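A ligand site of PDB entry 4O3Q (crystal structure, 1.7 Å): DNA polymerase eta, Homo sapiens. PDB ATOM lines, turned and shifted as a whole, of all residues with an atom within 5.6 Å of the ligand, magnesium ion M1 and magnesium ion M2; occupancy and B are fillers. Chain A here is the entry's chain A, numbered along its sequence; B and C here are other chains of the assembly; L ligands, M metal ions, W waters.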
ATOM      1  N   ASP A  16       0.724 -22.493  17.196  1.00  0.00           N
ATOM      2  CA  ASP A  16       0.797 -21.047  17.469  1.00  0.00           C
ATOM      3  C   ASP A  16       1.656 -20.316  16.421  1.00  0.00           C
ATOM      4  O   ASP A  16       2.803 -20.680  16.182  1.00  0.00           O
ATOM      5  CB  ASP A  16       1.365 -20.801  18.865  1.00  0.00           C
ATOM      6  CG  ASP A  16       1.357 -19.346  19.236  1.00  0.00           C
ATOM      7  OD1 ASP A  16       0.474 -18.925  20.002  1.00  0.00           O
ATOM      8  OD2 ASP A  16       2.240 -18.630  18.746  1.00  0.00           O
ATOM      9  N   MET A  17       1.098 -19.274  15.810  1.00  0.00           N
ATOM     10  CA  MET A  17       1.800 -18.569  14.757  1.00  0.00           C
ATOM     11  C   MET A  17       3.048 -17.884  15.309  1.00  0.00           C
ATOM     12  O   MET A  17       3.026 -17.343  16.415  1.00  0.00           O
ATOM     13  CB  MET A  17       0.878 -17.547  14.086  1.00  0.00           C
ATOM     14  CG  MET A  17      -0.450 -18.138  13.670  1.00  0.00           C
ATOM     15  SD  MET A  17      -0.275 -19.530  12.544  1.00  0.00           S
ATOM     16  CE  MET A  17       0.492 -18.769  11.160  1.00  0.00           C
ATOM     17  N   ASP A  18       4.131 -17.927  14.551  1.00  0.00           N
ATOM     18  CA  ASP A  18       5.354 -17.228  14.957  1.00  0.00           C
ATOM     19  C   ASP A  18       5.162 -15.728  14.742  1.00  0.00           C
ATOM     20  O   ASP A  18       4.650 -15.342  13.703  1.00  0.00           O
ATOM     21  CB  ASP A  18       6.563 -17.730  14.179  1.00  0.00           C
ATOM     22  CG  ASP A  18       6.822 -19.228  14.390  1.00  0.00           C
ATOM     23  OD1 ASP A  18       6.465 -19.768  15.462  1.00  0.00           O
ATOM     24  OD2 ASP A  18       7.368 -19.860  13.463  1.00  0.00           O
ATOM     25  N   CYS A  19       5.598 -14.909  15.700  1.00  0.00           N
ATOM     26  CA  CYS A  19       5.455 -13.442  15.650  1.00  0.00           C
ATOM     27  C   CYS A  19       4.324 -12.951  14.733  1.00  0.00           C
ATOM     28  O   CYS A  19       4.558 -12.242  13.737  1.00  0.00           O
ATOM     29  CB  CYS A  19       6.788 -12.783  15.256  1.00  0.00           C
ATOM     30  SG  CYS A  19       7.661 -13.361  13.784  1.00  0.00           S
ATOM     31  N   PHE A  20       3.107 -13.374  15.045  1.00  0.00           N
ATOM     32  CA  PHE A  20       2.004 -13.361  14.092  1.00  0.00           C
ATOM     33  C   PHE A  20       1.738 -12.003  13.415  1.00  0.00           C
ATOM     34  O   PHE A  20       1.705 -11.939  12.177  1.00  0.00           O
ATOM     35  CB  PHE A  20       0.715 -13.824  14.771  1.00  0.00           C
ATOM     36  CG  PHE A  20      -0.439 -13.978  13.824  1.00  0.00           C
ATOM     37  CD1 PHE A  20      -0.232 -14.560  12.575  1.00  0.00           C
ATOM     38  CD2 PHE A  20      -1.709 -13.565  14.173  1.00  0.00           C
ATOM     39  CE1 PHE A  20      -1.297 -14.733  11.688  1.00  0.00           C
ATOM     40  CE2 PHE A  20      -2.778 -13.720  13.278  1.00  0.00           C
ATOM     41  CZ  PHE A  20      -2.567 -14.319  12.038  1.00  0.00           C
ATOM     42  N   PHE A  21       1.537 -10.940  14.186  1.00  0.00           N
ATOM     43  CA  PHE A  21       1.182  -9.649  13.552  1.00  0.00           C
ATOM     44  C   PHE A  21       2.345  -9.179  12.669  1.00  0.00           C
ATOM     45  O   PHE A  21       2.119  -8.545  11.658  1.00  0.00           O
ATOM     46  CB  PHE A  21       0.832  -8.554  14.569  1.00  0.00           C
ATOM     47  CG  PHE A  21      -0.496  -8.729  15.272  1.00  0.00           C
ATOM     48  CD1 PHE A  21      -1.161  -9.949  15.310  1.00  0.00           C
ATOM     49  CD2 PHE A  21      -1.084  -7.642  15.896  1.00  0.00           C
ATOM     50  CE1 PHE A  21      -2.381 -10.084  15.978  1.00  0.00           C
ATOM     51  CE2 PHE A  21      -2.289  -7.761  16.565  1.00  0.00           C
ATOM     52  CZ  PHE A  21      -2.945  -8.978  16.607  1.00  0.00           C
ATOM     53  N   VAL A  22       3.590  -9.467  13.069  1.00  0.00           N
ATOM     54  CA  VAL A  22       4.753  -9.145  12.254  1.00  0.00           C
ATOM     55  C   VAL A  22       4.700  -9.907  10.916  1.00  0.00           C
ATOM     56  O   VAL A  22       4.913  -9.317   9.850  1.00  0.00           O
ATOM     57  CB  VAL A  22       6.091  -9.457  12.978  1.00  0.00           C
ATOM     58  CG1 VAL A  22       7.275  -9.463  11.972  1.00  0.00           C
ATOM     59  CG2 VAL A  22       6.336  -8.460  14.105  1.00  0.00           C
ATOM     60  N   GLN A  41       1.328  -0.148  18.390  1.00  0.00           N
ATOM     61  CA  GLN A  41       0.058   0.565  18.424  1.00  0.00           C
ATOM     62  C   GLN A  41       0.308   2.027  18.786  1.00  0.00           C
ATOM     63  O   GLN A  41       1.016   2.314  19.741  1.00  0.00           O
ATOM     64  CB  GLN A  41      -0.925  -0.060  19.418  1.00  0.00           C
ATOM     65  CG  GLN A  41      -1.280  -1.490  19.099  1.00  0.00           C
ATOM     66  CD  GLN A  41      -2.287  -2.077  20.091  1.00  0.00           C
ATOM     67  OE1 GLN A  41      -3.331  -2.607  19.693  1.00  0.00           O
ATOM     68  NE2 GLN A  41      -1.975  -2.001  21.372  1.00  0.00           N
ATOM     69  N   ILE A  51       3.662  -4.648  20.155  1.00  0.00           N
ATOM     70  CA  ILE A  51       2.891  -5.815  20.557  1.00  0.00           C
ATOM     71  C   ILE A  51       3.335  -7.120  19.878  1.00  0.00           C
ATOM     72  O   ILE A  51       2.839  -8.197  20.223  1.00  0.00           O
ATOM     73  CB  ILE A  51       1.398  -5.610  20.329  1.00  0.00           C
ATOM     74  CG1 ILE A  51       1.095  -5.220  18.883  1.00  0.00           C
ATOM     75  CG2 ILE A  51       0.851  -4.562  21.317  1.00  0.00           C
ATOM     76  CD1 ILE A  51      -0.415  -5.353  18.555  1.00  0.00           C
ATOM     77  N   ALA A  52       4.306  -7.035  18.969  1.00  0.00           N
ATOM     78  CA  ALA A  52       4.821  -8.212  18.263  1.00  0.00           C
ATOM     79  C   ALA A  52       6.193  -7.919  17.665  1.00  0.00           C
ATOM     80  O   ALA A  52       6.431  -6.817  17.187  1.00  0.00           O
ATOM     81  CB  ALA A  52       3.852  -8.661  17.165  1.00  0.00           C
ATOM     82  N   VAL A  53       7.079  -8.912  17.697  1.00  0.00           N
ATOM     83  CA  VAL A  53       8.498  -8.712  17.440  1.00  0.00           C
ATOM     84  C   VAL A  53       9.084  -9.869  16.630  1.00  0.00           C
ATOM     85  O   VAL A  53       8.984 -11.033  17.033  1.00  0.00           O
ATOM     86  CB  VAL A  53       9.295  -8.590  18.758  1.00  0.00           C
ATOM     87  CG1 VAL A  53      10.756  -8.270  18.474  1.00  0.00           C
ATOM     88  CG2 VAL A  53       8.676  -7.565  19.686  1.00  0.00           C
ATOM     89  N   TYR A  55      11.805 -12.466  15.095  1.00  0.00           N
ATOM     90  CA  TYR A  55      12.862 -13.169  15.801  1.00  0.00           C
ATOM     91  C   TYR A  55      14.223 -12.484  15.563  1.00  0.00           C
ATOM     92  O   TYR A  55      15.067 -12.462  16.449  1.00  0.00           O
ATOM     93  CB  TYR A  55      12.854 -14.639  15.428  1.00  0.00           C
ATOM     94  CG  TYR A  55      11.756 -15.363  16.206  1.00  0.00           C
ATOM     95  CD1 TYR A  55      10.427 -15.264  15.805  1.00  0.00           C
ATOM     96  CD2 TYR A  55      12.030 -16.073  17.363  1.00  0.00           C
ATOM     97  CE1 TYR A  55       9.404 -15.873  16.527  1.00  0.00           C
ATOM     98  CE2 TYR A  55      11.014 -16.684  18.101  1.00  0.00           C
ATOM     99  CZ  TYR A  55       9.704 -16.583  17.673  1.00  0.00           C
ATOM    100  OH  TYR A  55       8.684 -17.187  18.383  1.00  0.00           O
ATOM    101  N   ARG A  58      14.248  -9.823  18.111  1.00  0.00           N
ATOM    102  CA  ARG A  58      14.301 -10.367  19.474  1.00  0.00           C
ATOM    103  C   ARG A  58      15.752 -10.577  19.871  1.00  0.00           C
ATOM    104  O   ARG A  58      16.112 -10.450  21.050  1.00  0.00           O
ATOM    105  CB  ARG A  58      13.534 -11.683  19.595  1.00  0.00           C
ATOM    106  CG  ARG A  58      12.039 -11.545  19.416  1.00  0.00           C
ATOM    107  CD  ARG A  58      11.320 -12.861  19.630  1.00  0.00           C
ATOM    108  NE  ARG A  58       9.926 -12.774  19.166  1.00  0.00           N
ATOM    109  CZ  ARG A  58       8.985 -13.656  19.482  1.00  0.00           C
ATOM    110  NH1 ARG A  58       9.284 -14.695  20.262  1.00  0.00           N
ATOM    111  NH2 ARG A  58       7.757 -13.501  19.013  1.00  0.00           N
ATOM    112  N   ARG A  64       7.829  -7.483  23.369  1.00  0.00           N
ATOM    113  CA  ARG A  64       6.482  -7.017  23.650  1.00  0.00           C
ATOM    114  C   ARG A  64       6.483  -6.060  24.852  1.00  0.00           C
ATOM    115  O   ARG A  64       7.234  -6.265  25.806  1.00  0.00           O
ATOM    116  CB  ARG A  64       5.574  -8.228  23.909  1.00  0.00           C
ATOM    117  CG  ARG A  64       4.156  -7.876  24.200  1.00  0.00           C
ATOM    118  CD  ARG A  64       3.361  -9.080  24.651  1.00  0.00           C
ATOM    119  NE  ARG A  64       2.038  -8.667  25.093  1.00  0.00           N
ATOM    120  CZ  ARG A  64       1.752  -8.278  26.332  1.00  0.00           C
ATOM    121  NH1 ARG A  64       2.702  -8.287  27.269  1.00  0.00           N
ATOM    122  NH2 ARG A  64       0.523  -7.902  26.633  1.00  0.00           N
ATOM    123  N   LEU A  92      -7.874  -3.782  14.837  1.00  0.00           N
ATOM    124  CA  LEU A  92      -7.107  -5.018  14.590  1.00  0.00           C
ATOM    125  C   LEU A  92      -7.707  -5.906  13.498  1.00  0.00           C
ATOM    126  O   LEU A  92      -7.395  -7.098  13.428  1.00  0.00           O
ATOM    127  CB  LEU A  92      -6.961  -5.809  15.893  1.00  0.00           C
ATOM    128  CG  LEU A  92      -6.446  -4.977  17.072  1.00  0.00           C
ATOM    129  CD1 LEU A  92      -6.457  -5.781  18.352  1.00  0.00           C
ATOM    130  CD2 LEU A  92      -5.056  -4.464  16.773  1.00  0.00           C
ATOM    131  N   SER A 116      -6.743 -18.199  20.869  1.00  0.00           N
ATOM    132  CA  SER A 116      -6.310 -16.810  20.795  1.00  0.00           C
ATOM    133  C   SER A 116      -6.403 -16.358  19.355  1.00  0.00           C
ATOM    134  O   SER A 116      -6.783 -17.141  18.492  1.00  0.00           O
ATOM    135  CB  SER A 116      -4.879 -16.620  21.298  1.00  0.00           C
ATOM    136  OG  SER A 116      -3.943 -17.008  20.298  1.00  0.00           O
ATOM    137  N   ILE A 117      -6.001 -15.130  19.083  1.00  0.00           N
ATOM    138  CA  ILE A 117      -5.994 -14.664  17.697  1.00  0.00           C
ATOM    139  C   ILE A 117      -5.017 -15.495  16.818  1.00  0.00           C
ATOM    140  O   ILE A 117      -5.211 -15.583  15.598  1.00  0.00           O
ATOM    141  CB  ILE A 117      -5.626 -13.175  17.600  1.00  0.00           C
ATOM    142  CG1 ILE A 117      -5.980 -12.617  16.218  1.00  0.00           C
ATOM    143  CG2 ILE A 117      -4.149 -12.935  17.906  1.00  0.00           C
ATOM    144  CD1 ILE A 117      -6.287 -11.116  16.217  1.00  0.00           C
ATOM    145  N   ASP A 118      -4.005 -16.110  17.421  1.00  0.00           N
ATOM    146  CA  ASP A 118      -3.027 -16.830  16.582  1.00  0.00           C
ATOM    147  C   ASP A 118      -2.745 -18.280  16.973  1.00  0.00           C
ATOM    148  O   ASP A 118      -1.722 -18.845  16.565  1.00  0.00           O
ATOM    149  CB  ASP A 118      -1.707 -16.059  16.537  1.00  0.00           C
ATOM    150  CG  ASP A 118      -0.734 -16.460  17.661  1.00  0.00           C
ATOM    151  OD1 ASP A 118      -1.168 -16.751  18.811  1.00  0.00           O
ATOM    152  OD2 ASP A 118       0.483 -16.525  17.374  1.00  0.00           O
ATOM    153  N   GLU A 119      -3.620 -18.899  17.770  1.00  0.00           N
ATOM    154  CA  GLU A 119      -3.386 -20.306  18.086  1.00  0.00           C
ATOM    155  C   GLU A 119      -4.658 -21.085  18.299  1.00  0.00           C
ATOM    156  O   GLU A 119      -5.704 -20.515  18.635  1.00  0.00           O
ATOM    157  CB  GLU A 119      -2.524 -20.441  19.336  1.00  0.00           C
ATOM    158  CG  GLU A 119      -3.209 -20.114  20.632  1.00  0.00           C
ATOM    159  CD  GLU A 119      -2.256 -19.490  21.607  1.00  0.00           C
ATOM    160  OE1 GLU A 119      -1.869 -20.163  22.580  1.00  0.00           O
ATOM    161  OE2 GLU A 119      -1.862 -18.341  21.385  1.00  0.00           O
ATOM    162  N   LYS A 227       0.826 -26.892  24.759  1.00  0.00           N
ATOM    163  CA  LYS A 227       1.172 -25.468  24.771  1.00  0.00           C
ATOM    164  C   LYS A 227       2.618 -25.253  25.201  1.00  0.00           C
ATOM    165  O   LYS A 227       3.347 -24.482  24.569  1.00  0.00           O
ATOM    166  CB  LYS A 227       0.216 -24.700  25.696  1.00  0.00           C
ATOM    167  CG  LYS A 227       0.559 -23.214  25.882  1.00  0.00           C
ATOM    168  CD  LYS A 227       0.433 -22.391  24.588  1.00  0.00           C
ATOM    169  CE  LYS A 227       0.713 -20.899  24.859  1.00  0.00           C
ATOM    170  NZ  LYS A 227       0.781 -20.050  23.624  1.00  0.00           N
ATOM    171  N   LYS A 234      10.400 -22.691  19.245  1.00  0.00           N
ATOM    172  CA  LYS A 234      10.065 -21.591  18.330  1.00  0.00           C
ATOM    173  C   LYS A 234      11.346 -20.929  17.851  1.00  0.00           C
ATOM    174  O   LYS A 234      12.303 -20.831  18.610  1.00  0.00           O
ATOM    175  CB  LYS A 234       9.173 -20.552  19.016  1.00  0.00           C
ATOM    176  CG  LYS A 234       7.679 -20.840  18.920  1.00  0.00           C
ATOM    177  CD  LYS A 234       6.823 -19.759  19.584  1.00  0.00           C
ATOM    178  CE  LYS A 234       5.328 -19.915  19.202  1.00  0.00           C
ATOM    179  NZ  LYS A 234       5.023 -19.290  17.863  1.00  0.00           N
ATOM    180  P    DT B   3       3.646   2.950  31.604  1.00  0.00           P
ATOM    181  OP1  DT B   3       3.973   3.444  32.965  1.00  0.00           O
ATOM    182  OP2  DT B   3       4.713   2.350  30.760  1.00  0.00           O
ATOM    183  O5'  DT B   3       2.457   1.895  31.751  1.00  0.00           O
ATOM    184  C5'  DT B   3       2.306   0.863  30.787  1.00  0.00           C
ATOM    185  C4'  DT B   3       1.841   1.408  29.451  1.00  0.00           C
ATOM    186  O4'  DT B   3       2.321   0.545  28.383  1.00  0.00           O
ATOM    187  C3'  DT B   3       0.322   1.479  29.286  1.00  0.00           C
ATOM    188  O3'  DT B   3      -0.056   2.593  28.487  1.00  0.00           O
ATOM    189  C2'  DT B   3       0.041   0.180  28.553  1.00  0.00           C
ATOM    190  C1'  DT B   3       1.215   0.160  27.594  1.00  0.00           C
ATOM    191  N1   DT B   3       1.462  -1.185  27.013  1.00  0.00           N
ATOM    192  C2   DT B   3       1.466  -1.338  25.642  1.00  0.00           C
ATOM    193  O2   DT B   3       1.309  -0.413  24.868  1.00  0.00           O
ATOM    194  N3   DT B   3       1.682  -2.622  25.222  1.00  0.00           N
ATOM    195  C4   DT B   3       1.869  -3.751  26.007  1.00  0.00           C
ATOM    196  O4   DT B   3       2.051  -4.868  25.528  1.00  0.00           O
ATOM    197  C5   DT B   3       1.844  -3.506  27.437  1.00  0.00           C
ATOM    198  C7   DT B   3       2.033  -4.624  28.406  1.00  0.00           C
ATOM    199  C6   DT B   3       1.629  -2.255  27.859  1.00  0.00           C
ATOM    200  P   8OG B   4      -1.593   2.798  28.050  1.00  0.00           P
ATOM    201  OP1 8OG B   4      -2.489   2.370  29.198  1.00  0.00           O
ATOM    202  OP2 8OG B   4      -1.738   4.179  27.458  1.00  0.00           O
ATOM    203  O5' 8OG B   4      -1.847   1.712  26.883  1.00  0.00           O
ATOM    204  C5' 8OG B   4      -1.263   1.776  25.576  1.00  0.00           C
ATOM    205  C4' 8OG B   4      -2.113   0.866  24.690  1.00  0.00           C
ATOM    206  O4' 8OG B   4      -1.759  -0.516  24.748  1.00  0.00           O
ATOM    207  C3' 8OG B   4      -3.577   0.914  25.100  1.00  0.00           C
ATOM    208  O3' 8OG B   4      -4.254   1.059  23.853  1.00  0.00           O
ATOM    209  C2' 8OG B   4      -3.876  -0.439  25.717  1.00  0.00           C
ATOM    210  C1' 8OG B   4      -2.930  -1.324  24.926  1.00  0.00           C
ATOM    211  N9  8OG B   4      -2.443  -2.531  25.603  1.00  0.00           N
ATOM    212  C8  8OG B   4      -2.173  -3.672  24.988  1.00  0.00           C
ATOM    213  N7  8OG B   4      -1.691  -4.670  25.745  1.00  0.00           N
ATOM    214  C5  8OG B   4      -1.644  -4.121  26.975  1.00  0.00           C
ATOM    215  C6  8OG B   4      -1.231  -4.595  28.318  1.00  0.00           C
ATOM    216  O6  8OG B   4      -0.828  -5.756  28.479  1.00  0.00           O
ATOM    217  N1  8OG B   4      -1.328  -3.734  29.347  1.00  0.00           N
ATOM    218  C2  8OG B   4      -1.773  -2.474  29.197  1.00  0.00           C
ATOM    219  N2  8OG B   4      -1.837  -1.658  30.282  1.00  0.00           N
ATOM    220  N3  8OG B   4      -2.160  -1.965  28.006  1.00  0.00           N
ATOM    221  C4  8OG B   4      -2.115  -2.727  26.879  1.00  0.00           C
ATOM    222  O8  8OG B   4      -2.392  -3.775  23.726  1.00  0.00           O
ATOM    223  P    DA B   5      -5.847   0.867  23.743  1.00  0.00           P
ATOM    224  OP1  DA B   5      -6.296   1.750  22.646  1.00  0.00           O
ATOM    225  OP2  DA B   5      -6.480   0.980  25.064  1.00  0.00           O
ATOM    226  O5'  DA B   5      -5.992  -0.652  23.264  1.00  0.00           O
ATOM    227  C5'  DA B   5      -5.503  -1.030  21.978  1.00  0.00           C
ATOM    228  C4'  DA B   5      -6.039  -2.405  21.598  1.00  0.00           C
ATOM    229  O4'  DA B   5      -5.462  -3.427  22.469  1.00  0.00           O
ATOM    230  C3'  DA B   5      -7.541  -2.565  21.719  1.00  0.00           C
ATOM    231  O3'  DA B   5      -7.993  -3.438  20.703  1.00  0.00           O
ATOM    232  C2'  DA B   5      -7.710  -3.174  23.118  1.00  0.00           C
ATOM    233  C1'  DA B   5      -6.491  -4.082  23.194  1.00  0.00           C
ATOM    234  N9   DA B   5      -5.998  -4.305  24.549  1.00  0.00           N
ATOM    235  C8   DA B   5      -6.032  -3.420  25.598  1.00  0.00           C
ATOM    236  N7   DA B   5      -5.488  -3.889  26.708  1.00  0.00           N
ATOM    237  C5   DA B   5      -5.058  -5.149  26.357  1.00  0.00           C
ATOM    238  C6   DA B   5      -4.400  -6.152  27.094  1.00  0.00           C
ATOM    239  N6   DA B   5      -4.052  -6.015  28.368  1.00  0.00           N
ATOM    240  N1   DA B   5      -4.105  -7.303  26.448  1.00  0.00           N
ATOM    241  C2   DA B   5      -4.459  -7.438  25.158  1.00  0.00           C
ATOM    242  N3   DA B   5      -5.085  -6.558  24.366  1.00  0.00           N
ATOM    243  C4   DA B   5      -5.365  -5.430  25.027  1.00  0.00           C
ATOM    244  P    DT C   8       0.716 -16.112  27.994  1.00  0.00           P
ATOM    245  OP1  DT C   8       0.926 -17.355  27.202  1.00  0.00           O
ATOM    246  OP2  DT C   8       1.646 -15.692  29.072  1.00  0.00           O
ATOM    247  O5'  DT C   8       0.664 -14.881  26.987  1.00  0.00           O
ATOM    248  C5'  DT C   8      -0.056 -14.978  25.778  1.00  0.00           C
ATOM    249  C4'  DT C   8      -0.052 -13.637  25.084  1.00  0.00           C
ATOM    250  O4'  DT C   8      -0.941 -12.726  25.809  1.00  0.00           O
ATOM    251  C3'  DT C   8       1.328 -12.953  25.066  1.00  0.00           C
ATOM    252  O3'  DT C   8       1.617 -12.407  23.783  1.00  0.00           O
ATOM    253  C2'  DT C   8       1.179 -11.848  26.104  1.00  0.00           C
ATOM    254  C1'  DT C   8      -0.282 -11.498  25.882  1.00  0.00           C
ATOM    255  N1   DT C   8      -0.856 -10.679  26.946  1.00  0.00           N
ATOM    256  C2   DT C   8      -1.963  -9.916  26.663  1.00  0.00           C
ATOM    257  O2   DT C   8      -2.500  -9.923  25.576  1.00  0.00           O
ATOM    258  N3   DT C   8      -2.415  -9.148  27.687  1.00  0.00           N
ATOM    259  C4   DT C   8      -1.884  -9.075  28.956  1.00  0.00           C
ATOM    260  O4   DT C   8      -2.358  -8.345  29.820  1.00  0.00           O
ATOM    261  C5   DT C   8      -0.710  -9.889  29.198  1.00  0.00           C
ATOM    262  C7   DT C   8      -0.054  -9.888  30.542  1.00  0.00           C
ATOM    263  C6   DT C   8      -0.265 -10.660  28.195  1.00  0.00           C
HETATM  264  N1  LIG L   1      -2.224  -6.159  22.758  1.00  0.00           N
HETATM  265  C1  LIG L   1      -2.668  -6.353  21.436  1.00  0.00           C
HETATM  266  N2  LIG L   1      -3.594  -5.422  20.881  1.00  0.00           N
HETATM  267  N3  LIG L   1      -2.209  -7.480  20.672  1.00  0.00           N
HETATM  268  C2  LIG L   1      -1.258  -8.386  21.289  1.00  0.00           C
HETATM  269  C3  LIG L   1      -0.835  -8.211  22.561  1.00  0.00           C
HETATM  270  C4  LIG L   1      -1.337  -7.023  23.352  1.00  0.00           C
HETATM  271  O1  LIG L   1      -0.998  -6.832  24.484  1.00  0.00           O
HETATM  272  N4  LIG L   1       0.032  -9.218  22.872  1.00  0.00           N
HETATM  273  C5  LIG L   1       0.132 -10.006  21.781  1.00  0.00           C
HETATM  274  N5  LIG L   1      -0.676  -9.494  20.810  1.00  0.00           N
HETATM  275  P1  LIG L   1       1.578 -14.498  20.714  1.00  0.00           P
HETATM  276  P2  LIG L   1       3.642 -13.871  18.638  1.00  0.00           P
HETATM  277  P3  LIG L   1       5.405 -15.995  19.163  1.00  0.00           P
HETATM  278  C6  LIG L   1      -0.888  -9.953  19.467  1.00  0.00           C
HETATM  279  O2  LIG L   1       1.322 -15.850  20.071  1.00  0.00           O
HETATM  280  O3  LIG L   1       3.813 -12.455  18.135  1.00  0.00           O
HETATM  281  O4  LIG L   1       6.242 -16.512  18.037  1.00  0.00           O
HETATM  282  C7  LIG L   1       0.228  -9.830  18.754  1.00  0.00           C
HETATM  283  O5  LIG L   1       1.604 -14.558  22.240  1.00  0.00           O
HETATM  284  O6  LIG L   1       2.766 -14.723  17.764  1.00  0.00           O
HETATM  285  O7  LIG L   1       4.082 -16.728  19.239  1.00  0.00           O
HETATM  286  C8  LIG L   1       0.792 -11.325  18.511  1.00  0.00           C
HETATM  287  O8  LIG L   1       1.483 -11.349  17.253  1.00  0.00           O
HETATM  288  N6  LIG L   1       3.030 -13.757  20.203  1.00  0.00           N
HETATM  289  O9  LIG L   1       5.064 -14.500  18.797  1.00  0.00           O
HETATM  290  O10 LIG L   1       6.183 -15.971  20.452  1.00  0.00           O
HETATM  291  C9  LIG L   1      -0.324 -12.110  18.459  1.00  0.00           C
HETATM  292  O11 LIG L   1      -1.266 -11.490  19.448  1.00  0.00           O
HETATM  293  C10 LIG L   1      -0.058 -13.532  18.937  1.00  0.00           C
HETATM  294  O12 LIG L   1       0.397 -13.487  20.299  1.00  0.00           O
HETATM  295 MG    MG M   1       2.341 -16.676  18.306  1.00  0.00          MG
HETATM  296 MG    MG M   2      -0.287 -17.143  20.615  1.00  0.00          MG
HETATM  297  O   HOH W   1       5.992 -11.258  19.074  1.00  0.00           O
HETATM  298  O   HOH W   2       3.519 -15.706  23.961  1.00  0.00           O
HETATM  299  O   HOH W   3      -2.594 -13.110  21.532  1.00  0.00           O
HETATM  300  O   HOH W   4       3.629 -11.013  21.280  1.00  0.00           O
HETATM  301  O   HOH W   5       5.999 -14.299  22.404  1.00  0.00           O
HETATM  302  O   HOH W   6      -1.387 -15.616  21.670  1.00  0.00           O
HETATM  303  O   HOH W   7       0.884 -17.258  22.368  1.00  0.00           O
HETATM  304  O   HOH W   8       8.082 -17.414  21.951  1.00  0.00           O
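OH of Tyr 55 lies within hydrogen-bond range of O4 of the ligand (2.6 Å).
O8 of 8OG 4 of chain B is in hydrogen-bond range of a nitrogen (N1) of the ligand.
O3' of DT 8 of chain C sits close to an oxygen (O5) of the ligand, 2.6 Å away.
NH2 of Arg 64 sits at hydrogen-bond distance from O1 of the ligand, 2.8 Å away.
O10 of the ligand is in salt-bridge range of NH2 of Arg 58 (3.3 Å).
An oxygen (O4) of the ligand sits at hydrogen-bond distance from the backbone NH of Cys 19 (2.9 Å).
The side-chain amino group of Lys 234 lies within salt-bridge range of an oxygen (O4) of the ligand (3.0 Å).
The backbone NH (N) of Phe 20 is in hydrogen-bond range of an oxygen (O3) of the ligand (3.3 Å).
OE1 of Gln 41 is in hydrogen-bond range of N2 of the ligand, 3.1 Å away.
The backbone NH (N) of Phe 21 is in hydrogen-bond range of an oxygen (O8) of the ligand, 3.1 Å away.
O4' of DA 5 of chain B is in hydrogen-bond range of N2 of the ligand (3.2 Å).
N3 of DA 5 of chain B sits at hydrogen-bond distance from a nitrogen (N1) of the ligand.
The backbone carbonyl oxygen of Asp 16 lies within hydrogen-bond range of the side-chain amino group of Lys 234.
The side-chain amino group of Lys 234 lies close to the backbone carbonyl oxygen of Met 17 (3.1 Å).
The side-chain hydroxyl (OG) of Ser 116 lies within hydrogen-bond range of the backbone NH (N) of Glu 119, at 3.2 Å.
The side-chain amino group of Lys 227 lies within salt-bridge range of the side-chain carboxylate of Glu 119, 2.9 Å away.
NH1 of Arg 58 lies within hydrogen-bond range of OH of Tyr 55 (3.2 Å).
O6 of 8OG 4 of chain B lies within hydrogen-bond range of the guanidinium group (NH2) of Arg 64.
O8 of 8OG 4 of chain B is in hydrogen-bond range of NE2 of Gln 41 (3.0 Å).
The backbone carbonyl oxygen (O) of Val 53 is in hydrogen-bond range of the guanidinium group (NE) of Arg 58.
Residues that only touch the ligand: Asp 18 (3.3 Å), Ile 51 (3.4 Å), Ala 52 (3.6 Å), Leu 92 (3.8 Å), Ile 117 (3.6 Å) and DT 3 of chain B (3.8 Å).
Within 4 Å of the ligand: Asp 16, Met 17, Asp 18, Cys 19, Phe 20, Phe 21, Gln 41, Ile 51, Ala 52, Tyr 55, Arg 58, Arg 64, Leu 92, Ile 117, Asp 118, Lys 234, DT 3 of chain B, 8OG 4 of chain B, DA 5 of chain B and DT 8 of chain C.
The nearest printed residue that does not touch the ligand is Glu 119 (4.3 Å).
Residues that only touch magnesium ion M1: Lys 234.
Within 4 Å of magnesium ion M1: Asp 16, Met 17, Asp 118 and Lys 234.
The nearest printed residue that does not touch magnesium ion M1 is Asp 18 (4.3 Å).
Ser 116 touches magnesium ion M2.
Magnesium ion M1 is bound by O7 of the ligand (2.0 Å), OD2 of Asp 16 (2.0 Å), O6 of the ligand (2.1 Å), OD2 of Asp 118 (2.1 Å), O of Met 17 (2.1 Å) and O2 of the ligand (2.2 Å).
Magnesium ion M2 is bound by OD1 of Asp 16 (2.0 Å), OD1 of Asp 118 (2.0 Å), water W7 (2.1 Å), OE2 of Glu 119 (2.1 Å), O2 of the ligand (2.1 Å) and water W6 (2.2 Å).
Magnesium ion M2 has six donor atoms within binding distance.
Water W6 lies within hydrogen-bond range of O12 of the ligand (3.1 Å) and OG of Ser 116 (3.2 Å).
Water W7 bridges O5 of the ligand and NZ of Lys 227.
Water W1 lies within hydrogen-bond range of an oxygen (O3) of the ligand (2.7 Å), the guanidinium group of Arg 58 (2.9 Å) and the backbone NH of Val 53 (2.9 Å).
Water W8 bridges O10 of the ligand and NH1 of Arg 58.
Water W4 bridges N6 of the ligand (3.0 Å) and O of Ile 51 (3.1 Å).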
